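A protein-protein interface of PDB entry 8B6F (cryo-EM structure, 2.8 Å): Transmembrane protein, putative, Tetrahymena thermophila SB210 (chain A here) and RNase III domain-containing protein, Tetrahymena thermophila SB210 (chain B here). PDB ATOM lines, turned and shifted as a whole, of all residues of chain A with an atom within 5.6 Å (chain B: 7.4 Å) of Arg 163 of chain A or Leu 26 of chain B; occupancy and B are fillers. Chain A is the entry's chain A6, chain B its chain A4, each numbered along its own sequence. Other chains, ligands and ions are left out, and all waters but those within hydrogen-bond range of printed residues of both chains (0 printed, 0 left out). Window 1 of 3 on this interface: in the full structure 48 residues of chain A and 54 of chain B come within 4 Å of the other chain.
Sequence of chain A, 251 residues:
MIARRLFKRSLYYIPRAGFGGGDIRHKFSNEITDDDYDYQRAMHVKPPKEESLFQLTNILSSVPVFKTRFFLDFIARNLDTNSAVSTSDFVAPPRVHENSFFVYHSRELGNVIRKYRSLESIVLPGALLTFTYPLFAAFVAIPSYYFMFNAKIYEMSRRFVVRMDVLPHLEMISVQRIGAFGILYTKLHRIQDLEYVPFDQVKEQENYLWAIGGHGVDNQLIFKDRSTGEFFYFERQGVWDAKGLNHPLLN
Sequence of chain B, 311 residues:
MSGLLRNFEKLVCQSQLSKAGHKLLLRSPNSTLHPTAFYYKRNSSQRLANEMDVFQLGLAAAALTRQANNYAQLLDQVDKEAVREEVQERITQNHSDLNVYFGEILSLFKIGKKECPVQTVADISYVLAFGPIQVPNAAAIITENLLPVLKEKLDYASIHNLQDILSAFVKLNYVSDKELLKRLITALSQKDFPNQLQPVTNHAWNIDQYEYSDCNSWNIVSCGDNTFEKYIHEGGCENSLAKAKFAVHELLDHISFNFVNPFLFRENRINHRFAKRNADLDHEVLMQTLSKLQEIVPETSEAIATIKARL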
ATOM      1  N   PRO A  93      -1.942 -27.684  -2.690  1.00  0.00           N
ATOM      2  CA  PRO A  93      -0.905 -28.672  -2.990  1.00  0.00           C
ATOM      3  C   PRO A  93      -0.006 -28.898  -1.788  1.00  0.00           C
ATOM      4  O   PRO A  93       0.089 -28.034  -0.904  1.00  0.00           O
ATOM      5  CB  PRO A  93      -0.135 -28.038  -4.158  1.00  0.00           C
ATOM      6  CG  PRO A  93      -0.393 -26.588  -4.041  1.00  0.00           C
ATOM      7  CD  PRO A  93      -1.777 -26.455  -3.486  1.00  0.00           C
ATOM      8  N   PRO A  94       0.660 -30.051  -1.712  1.00  0.00           N
ATOM      9  CA  PRO A  94       1.510 -30.328  -0.548  1.00  0.00           C
ATOM     10  C   PRO A  94       2.581 -29.262  -0.375  1.00  0.00           C
ATOM     11  O   PRO A  94       3.177 -28.788  -1.343  1.00  0.00           O
ATOM     12  CB  PRO A  94       2.126 -31.694  -0.875  1.00  0.00           C
ATOM     13  CG  PRO A  94       1.231 -32.293  -1.898  1.00  0.00           C
ATOM     14  CD  PRO A  94       0.684 -31.151  -2.689  1.00  0.00           C
ATOM     15  N   ARG A  95       2.824 -28.887   0.878  1.00  0.00           N
ATOM     16  CA  ARG A  95       3.803 -27.850   1.169  1.00  0.00           C
ATOM     17  C   ARG A  95       5.204 -28.315   0.791  1.00  0.00           C
ATOM     18  O   ARG A  95       5.587 -29.461   1.042  1.00  0.00           O
ATOM     19  CB  ARG A  95       3.756 -27.471   2.649  1.00  0.00           C
ATOM     20  CG  ARG A  95       3.964 -28.637   3.604  1.00  0.00           C
ATOM     21  CD  ARG A  95       4.074 -28.161   5.044  1.00  0.00           C
ATOM     22  NE  ARG A  95       2.829 -27.583   5.538  1.00  0.00           N
ATOM     23  CZ  ARG A  95       1.898 -28.250   6.205  1.00  0.00           C
ATOM     24  NH1 ARG A  95       2.025 -29.538   6.474  1.00  0.00           N
ATOM     25  NH2 ARG A  95       0.808 -27.607   6.616  1.00  0.00           N
ATOM     26  N   VAL A  96       5.969 -27.416   0.170  1.00  0.00           N
ATOM     27  CA  VAL A  96       7.350 -27.731  -0.183  1.00  0.00           C
ATOM     28  C   VAL A  96       8.215 -27.807   1.068  1.00  0.00           C
ATOM     29  O   VAL A  96       9.102 -28.662   1.176  1.00  0.00           O
ATOM     30  CB  VAL A  96       7.887 -26.694  -1.186  1.00  0.00           C
ATOM     31  CG1 VAL A  96       9.371 -26.902  -1.439  1.00  0.00           C
ATOM     32  CG2 VAL A  96       7.117 -26.774  -2.491  1.00  0.00           C
ATOM     33  N   PHE A 102       2.129 -22.018  -0.111  1.00  0.00           N
ATOM     34  CA  PHE A 102       2.111 -21.905  -1.562  1.00  0.00           C
ATOM     35  C   PHE A 102       1.318 -20.680  -2.002  1.00  0.00           C
ATOM     36  O   PHE A 102       0.419 -20.211  -1.298  1.00  0.00           O
ATOM     37  CB  PHE A 102       1.520 -23.171  -2.186  1.00  0.00           C
ATOM     38  CG  PHE A 102       0.234 -22.945  -2.925  1.00  0.00           C
ATOM     39  CD1 PHE A 102      -0.975 -22.920  -2.252  1.00  0.00           C
ATOM     40  CD2 PHE A 102       0.233 -22.780  -4.301  1.00  0.00           C
ATOM     41  CE1 PHE A 102      -2.158 -22.718  -2.935  1.00  0.00           C
ATOM     42  CE2 PHE A 102      -0.945 -22.580  -4.989  1.00  0.00           C
ATOM     43  CZ  PHE A 102      -2.143 -22.549  -4.305  1.00  0.00           C
ATOM     44  N   TYR A 104       1.330 -19.772  -5.989  1.00  0.00           N
ATOM     45  CA  TYR A 104       0.983 -19.985  -7.386  1.00  0.00           C
ATOM     46  C   TYR A 104       1.352 -21.399  -7.809  1.00  0.00           C
ATOM     47  O   TYR A 104       2.328 -21.975  -7.321  1.00  0.00           O
ATOM     48  CB  TYR A 104       1.693 -18.967  -8.289  1.00  0.00           C
ATOM     49  CG  TYR A 104       1.763 -19.373  -9.742  1.00  0.00           C
ATOM     50  CD1 TYR A 104       0.671 -19.210 -10.584  1.00  0.00           C
ATOM     51  CD2 TYR A 104       2.924 -19.914 -10.273  1.00  0.00           C
ATOM     52  CE1 TYR A 104       0.736 -19.579 -11.915  1.00  0.00           C
ATOM     53  CE2 TYR A 104       2.999 -20.284 -11.599  1.00  0.00           C
ATOM     54  CZ  TYR A 104       1.903 -20.115 -12.414  1.00  0.00           C
ATOM     55  OH  TYR A 104       1.980 -20.486 -13.734  1.00  0.00           O
ATOM     56  N   HIS A 105       0.561 -21.952  -8.727  1.00  0.00           N
ATOM     57  CA  HIS A 105       0.803 -23.288  -9.249  1.00  0.00           C
ATOM     58  C   HIS A 105       0.232 -23.372 -10.658  1.00  0.00           C
ATOM     59  O   HIS A 105      -0.824 -22.801 -10.940  1.00  0.00           O
ATOM     60  CB  HIS A 105       0.171 -24.353  -8.347  1.00  0.00           C
ATOM     61  CG  HIS A 105       0.643 -25.745  -8.633  1.00  0.00           C
ATOM     62  ND1 HIS A 105       0.177 -26.484  -9.699  1.00  0.00           N
ATOM     63  CD2 HIS A 105       1.531 -26.534  -7.986  1.00  0.00           C
ATOM     64  CE1 HIS A 105       0.765 -27.667  -9.699  1.00  0.00           C
ATOM     65  NE2 HIS A 105       1.590 -27.724  -8.670  1.00  0.00           N
ATOM     66  N   SER A 106       0.930 -24.090 -11.535  1.00  0.00           N
ATOM     67  CA  SER A 106       0.530 -24.243 -12.929  1.00  0.00           C
ATOM     68  C   SER A 106      -0.086 -25.621 -13.132  1.00  0.00           C
ATOM     69  O   SER A 106       0.470 -26.625 -12.678  1.00  0.00           O
ATOM     70  CB  SER A 106       1.724 -24.054 -13.863  1.00  0.00           C
ATOM     71  OG  SER A 106       2.741 -24.997 -13.582  1.00  0.00           O
ATOM     72  N   VAL A 161       7.380 -20.935 -14.587  1.00  0.00           N
ATOM     73  CA  VAL A 161       7.290 -21.212 -13.158  1.00  0.00           C
ATOM     74  C   VAL A 161       6.246 -22.298 -12.955  1.00  0.00           C
ATOM     75  O   VAL A 161       5.045 -22.064 -13.126  1.00  0.00           O
ATOM     76  CB  VAL A 161       6.941 -19.949 -12.361  1.00  0.00           C
ATOM     77  CG1 VAL A 161       6.628 -20.294 -10.913  1.00  0.00           C
ATOM     78  CG2 VAL A 161       8.084 -18.952 -12.429  1.00  0.00           C
ATOM     79  N   VAL A 162       6.708 -23.495 -12.594  1.00  0.00           N
ATOM     80  CA  VAL A 162       5.787 -24.592 -12.324  1.00  0.00           C
ATOM     81  C   VAL A 162       5.022 -24.341 -11.032  1.00  0.00           C
ATOM     82  O   VAL A 162       3.801 -24.520 -10.968  1.00  0.00           O
ATOM     83  CB  VAL A 162       6.551 -25.927 -12.277  1.00  0.00           C
ATOM     84  CG1 VAL A 162       5.772 -26.969 -11.493  1.00  0.00           C
ATOM     85  CG2 VAL A 162       6.830 -26.420 -13.678  1.00  0.00           C
ATOM     86  N   ARG A 163       5.727 -23.917  -9.989  1.00  0.00           N
ATOM     87  CA  ARG A 163       5.117 -23.692  -8.691  1.00  0.00           C
ATOM     88  C   ARG A 163       5.890 -22.607  -7.960  1.00  0.00           C
ATOM     89  O   ARG A 163       7.092 -22.431  -8.178  1.00  0.00           O
ATOM     90  CB  ARG A 163       5.087 -24.982  -7.863  1.00  0.00           C
ATOM     91  CG  ARG A 163       4.626 -24.785  -6.434  1.00  0.00           C
ATOM     92  CD  ARG A 163       4.487 -26.104  -5.701  1.00  0.00           C
ATOM     93  NE  ARG A 163       4.008 -25.892  -4.341  1.00  0.00           N
ATOM     94  CZ  ARG A 163       3.683 -26.859  -3.497  1.00  0.00           C
ATOM     95  NH1 ARG A 163       3.769 -28.133  -3.837  1.00  0.00           N
ATOM     96  NH2 ARG A 163       3.253 -26.538  -2.279  1.00  0.00           N
ATOM     97  N   MET A 164       5.190 -21.873  -7.100  1.00  0.00           N
ATOM     98  CA  MET A 164       5.807 -20.825  -6.298  1.00  0.00           C
ATOM     99  C   MET A 164       5.282 -20.928  -4.876  1.00  0.00           C
ATOM    100  O   MET A 164       4.067 -20.899  -4.660  1.00  0.00           O
ATOM    101  CB  MET A 164       5.517 -19.440  -6.880  1.00  0.00           C
ATOM    102  CG  MET A 164       6.304 -18.327  -6.211  1.00  0.00           C
ATOM    103  SD  MET A 164       6.098 -16.721  -7.004  1.00  0.00           S
ATOM    104  CE  MET A 164       4.357 -16.422  -6.721  1.00  0.00           C
ATOM    105  N   ASP A 165       6.194 -21.044  -3.915  1.00  0.00           N
ATOM    106  CA  ASP A 165       5.869 -21.015  -2.497  1.00  0.00           C
ATOM    107  C   ASP A 165       6.715 -19.944  -1.826  1.00  0.00           C
ATOM    108  O   ASP A 165       7.695 -19.455  -2.391  1.00  0.00           O
ATOM    109  CB  ASP A 165       6.103 -22.376  -1.827  1.00  0.00           C
ATOM    110  CG  ASP A 165       5.178 -23.453  -2.354  1.00  0.00           C
ATOM    111  OD1 ASP A 165       4.515 -23.221  -3.386  1.00  0.00           O
ATOM    112  OD2 ASP A 165       5.102 -24.531  -1.731  1.00  0.00           O
ATOM    113  N   SER A 174      10.416 -19.926  -3.053  1.00  0.00           N
ATOM    114  CA  SER A 174      10.904 -21.117  -3.736  1.00  0.00           C
ATOM    115  C   SER A 174      10.130 -21.281  -5.036  1.00  0.00           C
ATOM    116  O   SER A 174       8.896 -21.331  -5.027  1.00  0.00           O
ATOM    117  CB  SER A 174      10.751 -22.358  -2.858  1.00  0.00           C
ATOM    118  OG  SER A 174       9.387 -22.632  -2.598  1.00  0.00           O
ATOM    119  N   VAL A 175      10.860 -21.363  -6.145  1.00  0.00           N
ATOM    120  CA  VAL A 175      10.284 -21.486  -7.477  1.00  0.00           C
ATOM    121  C   VAL A 175      10.733 -22.813  -8.070  1.00  0.00           C
ATOM    122  O   VAL A 175      11.928 -23.123  -8.080  1.00  0.00           O
ATOM    123  CB  VAL A 175      10.715 -20.312  -8.376  1.00  0.00           C
ATOM    124  CG1 VAL A 175      10.157 -20.466  -9.769  1.00  0.00           C
ATOM    125  CG2 VAL A 175      10.267 -18.993  -7.776  1.00  0.00           C
ATOM    126  N   GLN A 176       9.772 -23.589  -8.565  1.00  0.00           N
ATOM    127  CA  GLN A 176      10.036 -24.880  -9.184  1.00  0.00           C
ATOM    128  C   GLN A 176      10.038 -24.734 -10.700  1.00  0.00           C
ATOM    129  O   GLN A 176       9.177 -24.058 -11.269  1.00  0.00           O
ATOM    130  CB  GLN A 176       8.993 -25.911  -8.757  1.00  0.00           C
ATOM    131  CG  GLN A 176       9.307 -27.325  -9.205  1.00  0.00           C
ATOM    132  CD  GLN A 176       8.285 -28.326  -8.716  1.00  0.00           C
ATOM    133  OE1 GLN A 176       7.159 -27.966  -8.380  1.00  0.00           O
ATOM    134  NE2 GLN A 176       8.677 -29.593  -8.664  1.00  0.00           N
ATOM    135  N   LEU B  24       0.492 -32.695   4.201  1.00  0.00           N
ATOM    136  CA  LEU B  24       1.216 -33.383   3.140  1.00  0.00           C
ATOM    137  C   LEU B  24       2.475 -32.599   2.806  1.00  0.00           C
ATOM    138  O   LEU B  24       2.420 -31.377   2.629  1.00  0.00           O
ATOM    139  CB  LEU B  24       0.351 -33.544   1.887  1.00  0.00           C
ATOM    140  CG  LEU B  24      -0.854 -34.481   1.998  1.00  0.00           C
ATOM    141  CD1 LEU B  24      -1.679 -34.438   0.724  1.00  0.00           C
ATOM    142  CD2 LEU B  24      -0.412 -35.903   2.291  1.00  0.00           C
ATOM    143  N   LEU B  25       3.599 -33.302   2.716  1.00  0.00           N
ATOM    144  CA  LEU B  25       4.889 -32.708   2.400  1.00  0.00           C
ATOM    145  C   LEU B  25       5.347 -33.192   1.033  1.00  0.00           C
ATOM    146  O   LEU B  25       5.165 -34.363   0.688  1.00  0.00           O
ATOM    147  CB  LEU B  25       5.930 -33.070   3.462  1.00  0.00           C
ATOM    148  CG  LEU B  25       7.321 -32.457   3.294  1.00  0.00           C
ATOM    149  CD1 LEU B  25       7.286 -30.960   3.545  1.00  0.00           C
ATOM    150  CD2 LEU B  25       8.313 -33.136   4.221  1.00  0.00           C
ATOM    151  N   LEU B  26       5.945 -32.291   0.259  1.00  0.00           N
ATOM    152  CA  LEU B  26       6.395 -32.594  -1.093  1.00  0.00           C
ATOM    153  C   LEU B  26       7.906 -32.782  -1.111  1.00  0.00           C
ATOM    154  O   LEU B  26       8.652 -31.902  -0.669  1.00  0.00           O
ATOM    155  CB  LEU B  26       5.998 -31.478  -2.062  1.00  0.00           C
ATOM    156  CG  LEU B  26       6.421 -31.672  -3.521  1.00  0.00           C
ATOM    157  CD1 LEU B  26       5.782 -32.917  -4.118  1.00  0.00           C
ATOM    158  CD2 LEU B  26       6.070 -30.444  -4.344  1.00  0.00           C
ATOM    159  N   ARG B  27       8.348 -33.927  -1.621  1.00  0.00           N
ATOM    160  CA  ARG B  27       9.760 -34.203  -1.852  1.00  0.00           C
ATOM    161  C   ARG B  27       9.984 -34.306  -3.353  1.00  0.00           C
ATOM    162  O   ARG B  27       9.464 -35.221  -4.000  1.00  0.00           O
ATOM    163  CB  ARG B  27      10.191 -35.494  -1.155  1.00  0.00           C
ATOM    164  CG  ARG B  27      10.188 -35.409   0.362  1.00  0.00           C
ATOM    165  CD  ARG B  27      10.592 -36.735   0.985  1.00  0.00           C
ATOM    166  NE  ARG B  27      10.576 -36.680   2.442  1.00  0.00           N
ATOM    167  CZ  ARG B  27      10.787 -37.722   3.235  1.00  0.00           C
ATOM    168  NH1 ARG B  27      11.030 -38.926   2.744  1.00  0.00           N
ATOM    169  NH2 ARG B  27      10.751 -37.551   4.553  1.00  0.00           N
ATOM    170  N   SER B  28      10.761 -33.379  -3.900  1.00  0.00           N
ATOM    171  CA  SER B  28      10.999 -33.313  -5.330  1.00  0.00           C
ATOM    172  C   SER B  28      12.492 -33.330  -5.612  1.00  0.00           C
ATOM    173  O   SER B  28      13.290 -32.901  -4.773  1.00  0.00           O
ATOM    174  CB  SER B  28      10.375 -32.048  -5.938  1.00  0.00           C
ATOM    175  OG  SER B  28      10.846 -30.882  -5.283  1.00  0.00           O
ATOM    176  N   SER B  31      15.905 -30.279  -5.089  1.00  0.00           N
ATOM    177  CA  SER B  31      15.256 -29.278  -4.254  1.00  0.00           C
ATOM    178  C   SER B  31      16.267 -28.731  -3.255  1.00  0.00           C
ATOM    179  O   SER B  31      16.854 -29.494  -2.479  1.00  0.00           O
ATOM    180  CB  SER B  31      14.050 -29.873  -3.528  1.00  0.00           C
ATOM    181  OG  SER B  31      14.434 -30.973  -2.721  1.00  0.00           O
ATOM    182  N   LEU B  33      16.082 -26.033  -0.437  1.00  0.00           N
ATOM    183  CA  LEU B  33      15.254 -25.148   0.369  1.00  0.00           C
ATOM    184  C   LEU B  33      16.033 -24.432   1.463  1.00  0.00           C
ATOM    185  O   LEU B  33      15.428 -23.702   2.253  1.00  0.00           O
ATOM    186  CB  LEU B  33      14.105 -25.942   0.997  1.00  0.00           C
ATOM    187  CG  LEU B  33      13.208 -26.690   0.008  1.00  0.00           C
ATOM    188  CD1 LEU B  33      12.143 -27.478   0.750  1.00  0.00           C
ATOM    189  CD2 LEU B  33      12.572 -25.732  -0.987  1.00  0.00           C
ATOM    190  N   GLN B 198       3.575 -36.079   5.970  1.00  0.00           N
ATOM    191  CA  GLN B 198       3.504 -37.240   5.088  1.00  0.00           C
ATOM    192  C   GLN B 198       4.146 -36.906   3.747  1.00  0.00           C
ATOM    193  O   GLN B 198       3.547 -36.165   2.953  1.00  0.00           O
ATOM    194  CB  GLN B 198       2.048 -37.663   4.890  1.00  0.00           C
ATOM    195  CG  GLN B 198       1.318 -37.968   6.190  1.00  0.00           C
ATOM    196  CD  GLN B 198      -0.153 -38.264   5.980  1.00  0.00           C
ATOM    197  OE1 GLN B 198      -0.652 -38.223   4.856  1.00  0.00           O
ATOM    198  NE2 GLN B 198      -0.858 -38.561   7.066  1.00  0.00           N
ATOM    199  N   PRO B 199       5.338 -37.415   3.439  1.00  0.00           N
ATOM    200  CA  PRO B 199       5.981 -37.054   2.170  1.00  0.00           C
ATOM    201  C   PRO B 199       5.240 -37.610   0.964  1.00  0.00           C
ATOM    202  O   PRO B 199       4.582 -38.652   1.033  1.00  0.00           O
ATOM    203  CB  PRO B 199       7.378 -37.673   2.293  1.00  0.00           C
ATOM    204  CG  PRO B 199       7.204 -38.803   3.240  1.00  0.00           C
ATOM    205  CD  PRO B 199       6.153 -38.364   4.216  1.00  0.00           C
ATOM    206  N   VAL B 200       5.352 -36.892  -0.156  1.00  0.00           N
ATOM    207  CA  VAL B 200       4.797 -37.323  -1.433  1.00  0.00           C
ATOM    208  C   VAL B 200       5.734 -36.875  -2.550  1.00  0.00           C
ATOM    209  O   VAL B 200       6.593 -36.011  -2.362  1.00  0.00           O
ATOM    210  CB  VAL B 200       3.370 -36.771  -1.678  1.00  0.00           C
ATOM    211  CG1 VAL B 200       2.467 -37.067  -0.491  1.00  0.00           C
ATOM    212  CG2 VAL B 200       3.398 -35.275  -1.968  1.00  0.00           C
ATOM    213  N   THR B 201       5.559 -37.478  -3.725  1.00  0.00           N
ATOM    214  CA  THR B 201       6.387 -37.180  -4.885  1.00  0.00           C
ATOM    215  C   THR B 201       5.515 -37.129  -6.131  1.00  0.00           C
ATOM    216  O   THR B 201       4.454 -37.755  -6.189  1.00  0.00           O
ATOM    217  CB  THR B 201       7.507 -38.219  -5.070  1.00  0.00           C
ATOM    218  OG1 THR B 201       8.245 -38.357  -3.849  1.00  0.00           O
ATOM    219  CG2 THR B 201       8.465 -37.805  -6.182  1.00  0.00           C
ATOM    220  N   ASN B 202       5.974 -36.375  -7.129  1.00  0.00           N
ATOM    221  CA  ASN B 202       5.225 -36.234  -8.370  1.00  0.00           C
ATOM    222  C   ASN B 202       5.076 -37.589  -9.052  1.00  0.00           C
ATOM    223  O   ASN B 202       5.919 -38.479  -8.910  1.00  0.00           O
ATOM    224  CB  ASN B 202       5.924 -35.248  -9.306  1.00  0.00           C
ATOM    225  CG  ASN B 202       6.034 -33.861  -8.711  1.00  0.00           C
ATOM    226  OD1 ASN B 202       7.032 -33.522  -8.078  1.00  0.00           O
ATOM    227  ND2 ASN B 202       5.000 -33.049  -8.908  1.00  0.00           N
ATOM    228  N   ILE B 207       2.606 -32.807 -12.674  1.00  0.00           N
ATOM    229  CA  ILE B 207       2.917 -31.939 -11.546  1.00  0.00           C
ATOM    230  C   ILE B 207       1.799 -31.986 -10.512  1.00  0.00           C
ATOM    231  O   ILE B 207       2.053 -31.986  -9.302  1.00  0.00           O
ATOM    232  CB  ILE B 207       3.168 -30.508 -12.050  1.00  0.00           C
ATOM    233  CG1 ILE B 207       4.322 -30.505 -13.056  1.00  0.00           C
ATOM    234  CG2 ILE B 207       3.477 -29.583 -10.884  1.00  0.00           C
ATOM    235  CD1 ILE B 207       4.370 -29.274 -13.920  1.00  0.00           C
ATOM    236  N   GLN B 209      -0.377 -34.427  -9.872  1.00  0.00           N
ATOM    237  CA  GLN B 209      -0.632 -35.732  -9.278  1.00  0.00           C
ATOM    238  C   GLN B 209       0.547 -36.161  -8.415  1.00  0.00           C
ATOM    239  O   GLN B 209       1.697 -36.134  -8.865  1.00  0.00           O
ATOM    240  CB  GLN B 209      -0.899 -36.770 -10.368  1.00  0.00           C
ATOM    241  CG  GLN B 209      -1.952 -36.333 -11.374  1.00  0.00           C
ATOM    242  CD  GLN B 209      -3.248 -35.912 -10.717  1.00  0.00           C
ATOM    243  OE1 GLN B 209      -3.587 -36.377  -9.630  1.00  0.00           O
ATOM    244  NE2 GLN B 209      -3.979 -35.019 -11.372  1.00  0.00           N
ATOM    245  N   TYR B 210       0.254 -36.557  -7.179  1.00  0.00           N
ATOM    246  CA  TYR B 210       1.265 -36.935  -6.204  1.00  0.00           C
ATOM    247  C   TYR B 210       0.995 -38.338  -5.675  1.00  0.00           C
ATOM    248  O   TYR B 210      -0.153 -38.782  -5.603  1.00  0.00           O
ATOM    249  CB  TYR B 210       1.297 -35.947  -5.035  1.00  0.00           C
ATOM    250  CG  TYR B 210       1.466 -34.506  -5.456  1.00  0.00           C
ATOM    251  CD1 TYR B 210       2.714 -34.009  -5.805  1.00  0.00           C
ATOM    252  CD2 TYR B 210       0.381 -33.644  -5.497  1.00  0.00           C
ATOM    253  CE1 TYR B 210       2.876 -32.692  -6.186  1.00  0.00           C
ATOM    254  CE2 TYR B 210       0.532 -32.325  -5.877  1.00  0.00           C
ATOM    255  CZ  TYR B 210       1.782 -31.855  -6.220  1.00  0.00           C
ATOM    256  OH  TYR B 210       1.943 -30.544  -6.599  1.00  0.00           O
ATOM    257  N   GLU B 211       2.072 -39.029  -5.302  1.00  0.00           N
ATOM    258  CA  GLU B 211       2.005 -40.375  -4.752  1.00  0.00           C
ATOM    259  C   GLU B 211       2.786 -40.426  -3.448  1.00  0.00           C
ATOM    260  O   GLU B 211       3.834 -39.788  -3.320  1.00  0.00           O
ATOM    261  CB  GLU B 211       2.578 -41.412  -5.726  1.00  0.00           C
ATOM    262  CG  GLU B 211       1.690 -41.712  -6.917  1.00  0.00           C
ATOM    263  CD  GLU B 211       2.388 -42.555  -7.968  1.00  0.00           C
ATOM    264  OE1 GLU B 211       3.611 -42.773  -7.840  1.00  0.00           O
ATOM    265  OE2 GLU B 211       1.715 -43.002  -8.920  1.00  0.00           O
ATOM    266  N   SER B 217      14.387 -38.060  -2.798  1.00  0.00           N
ATOM    267  CA  SER B 217      14.621 -37.799  -4.210  1.00  0.00           C
ATOM    268  C   SER B 217      16.044 -37.307  -4.427  1.00  0.00           C
ATOM    269  O   SER B 217      16.591 -36.562  -3.610  1.00  0.00           O
ATOM    270  CB  SER B 217      13.627 -36.766  -4.741  1.00  0.00           C
ATOM    271  OG  SER B 217      12.297 -37.247  -4.659  1.00  0.00           O
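Of chain B, only Leu 26 comes within 4 Å of Arg 163 of chain A.
Leu 26 of chain B touches just these residues of chain A: Pro 94 (3.96 Å), Arg 95 (3.0 Å), Val 96 (3.8 Å) and Arg 163 (3.3 Å).
Of the printed residues of chain B, His 105 of chain A touches Ile 207 and Tyr 210.
Printed residues of chain A within 4 Å of Ile 207 of chain B: His 105 (3.5 Å) and Val 162 (3.5 Å).
Of the printed residues of chain B, Val 96 of chain A touches Leu 25, Leu 26 and Leu 33.
Of the printed residues of chain B, Arg 95 of chain A touches Leu 24, Leu 25 and Leu 26.
The backbone NH of Arg 95 of chain A sits at hydrogen-bond distance from the backbone carbonyl oxygen of Leu 24 of chain B.
The backbone NH (N) of Leu 26 of chain B lies within hydrogen-bond range of the backbone carbonyl oxygen (O) of Arg 95 of chain A (3.0 Å).
Pro 94 of chain A touches Leu 24 of chain B.
Pro 94 of chain A touches Val 200 of chain B (CG to CG2, 3.7 Å).
Tyr 210 of chain B touches Pro 94 of chain A.
CD1 of Leu 25 of chain B touches O of Arg 95 of chain A (3.4 Å).
O of Val 96 of chain A touches CD1 of Leu 25 of chain B (3.8 Å).
Val 96 of chain A touches Leu 33 of chain B (O to CD1, 3.3 Å).
His 105 of chain A touches Ile 207 of chain B (NE2 to CG2, 3.5 Å).
OH of Tyr 210 of chain B touches NE2 of His 105 of chain A, 3.5 Å away.
Val 162 of chain A touches Ile 207 of chain B (CG1 to CG2, 3.5 Å).
Leu 26 of chain B touches Arg 163 of chain A.
Printed residues of chain A that touch a printed residue of chain B: Pro 94, Arg 95, Val 96, His 105, Val 162 and Arg 163.
Hydrophobic or aromatic side chains of chain A within 4 Å of the printed part of chain B: Pro 94, Val 96, His 105 and Val 162.
Among the printed residues, 14 pairs touch across the chains.
Among the printed residues, no Asp or Glu carboxylate lies within 4 Å of a Lys or Arg side-chain nitrogen of the other chain.
The backbone carbonyl oxygen of Gln 198 of chain B lies within hydrogen-bond range of the backbone NH of Leu 25 of chain B (2.9 Å).
The backbone NH of Val 200 of chain B lies within hydrogen-bond range of the backbone carbonyl oxygen of Leu 25 of chain B (2.7 Å).
O of Ile 207 of chain B is in hydrogen-bond range of OH of Tyr 210 of chain B, at 3.1 Å.
The backbone carbonyl oxygen (O) of Pro 94 of chain A sits at hydrogen-bond distance from the guanidinium group (NH2) of Arg 163 of chain A (2.4 Å).
N of Val 162 of chain A is in hydrogen-bond range of O of Gln 176 of chain A, 2.9 Å away.
The guanidinium group (NH2) of Arg 163 of chain A is in salt-bridge range of the side-chain carboxylate (OD2) of Asp 165 of chain A (2.8 Å).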
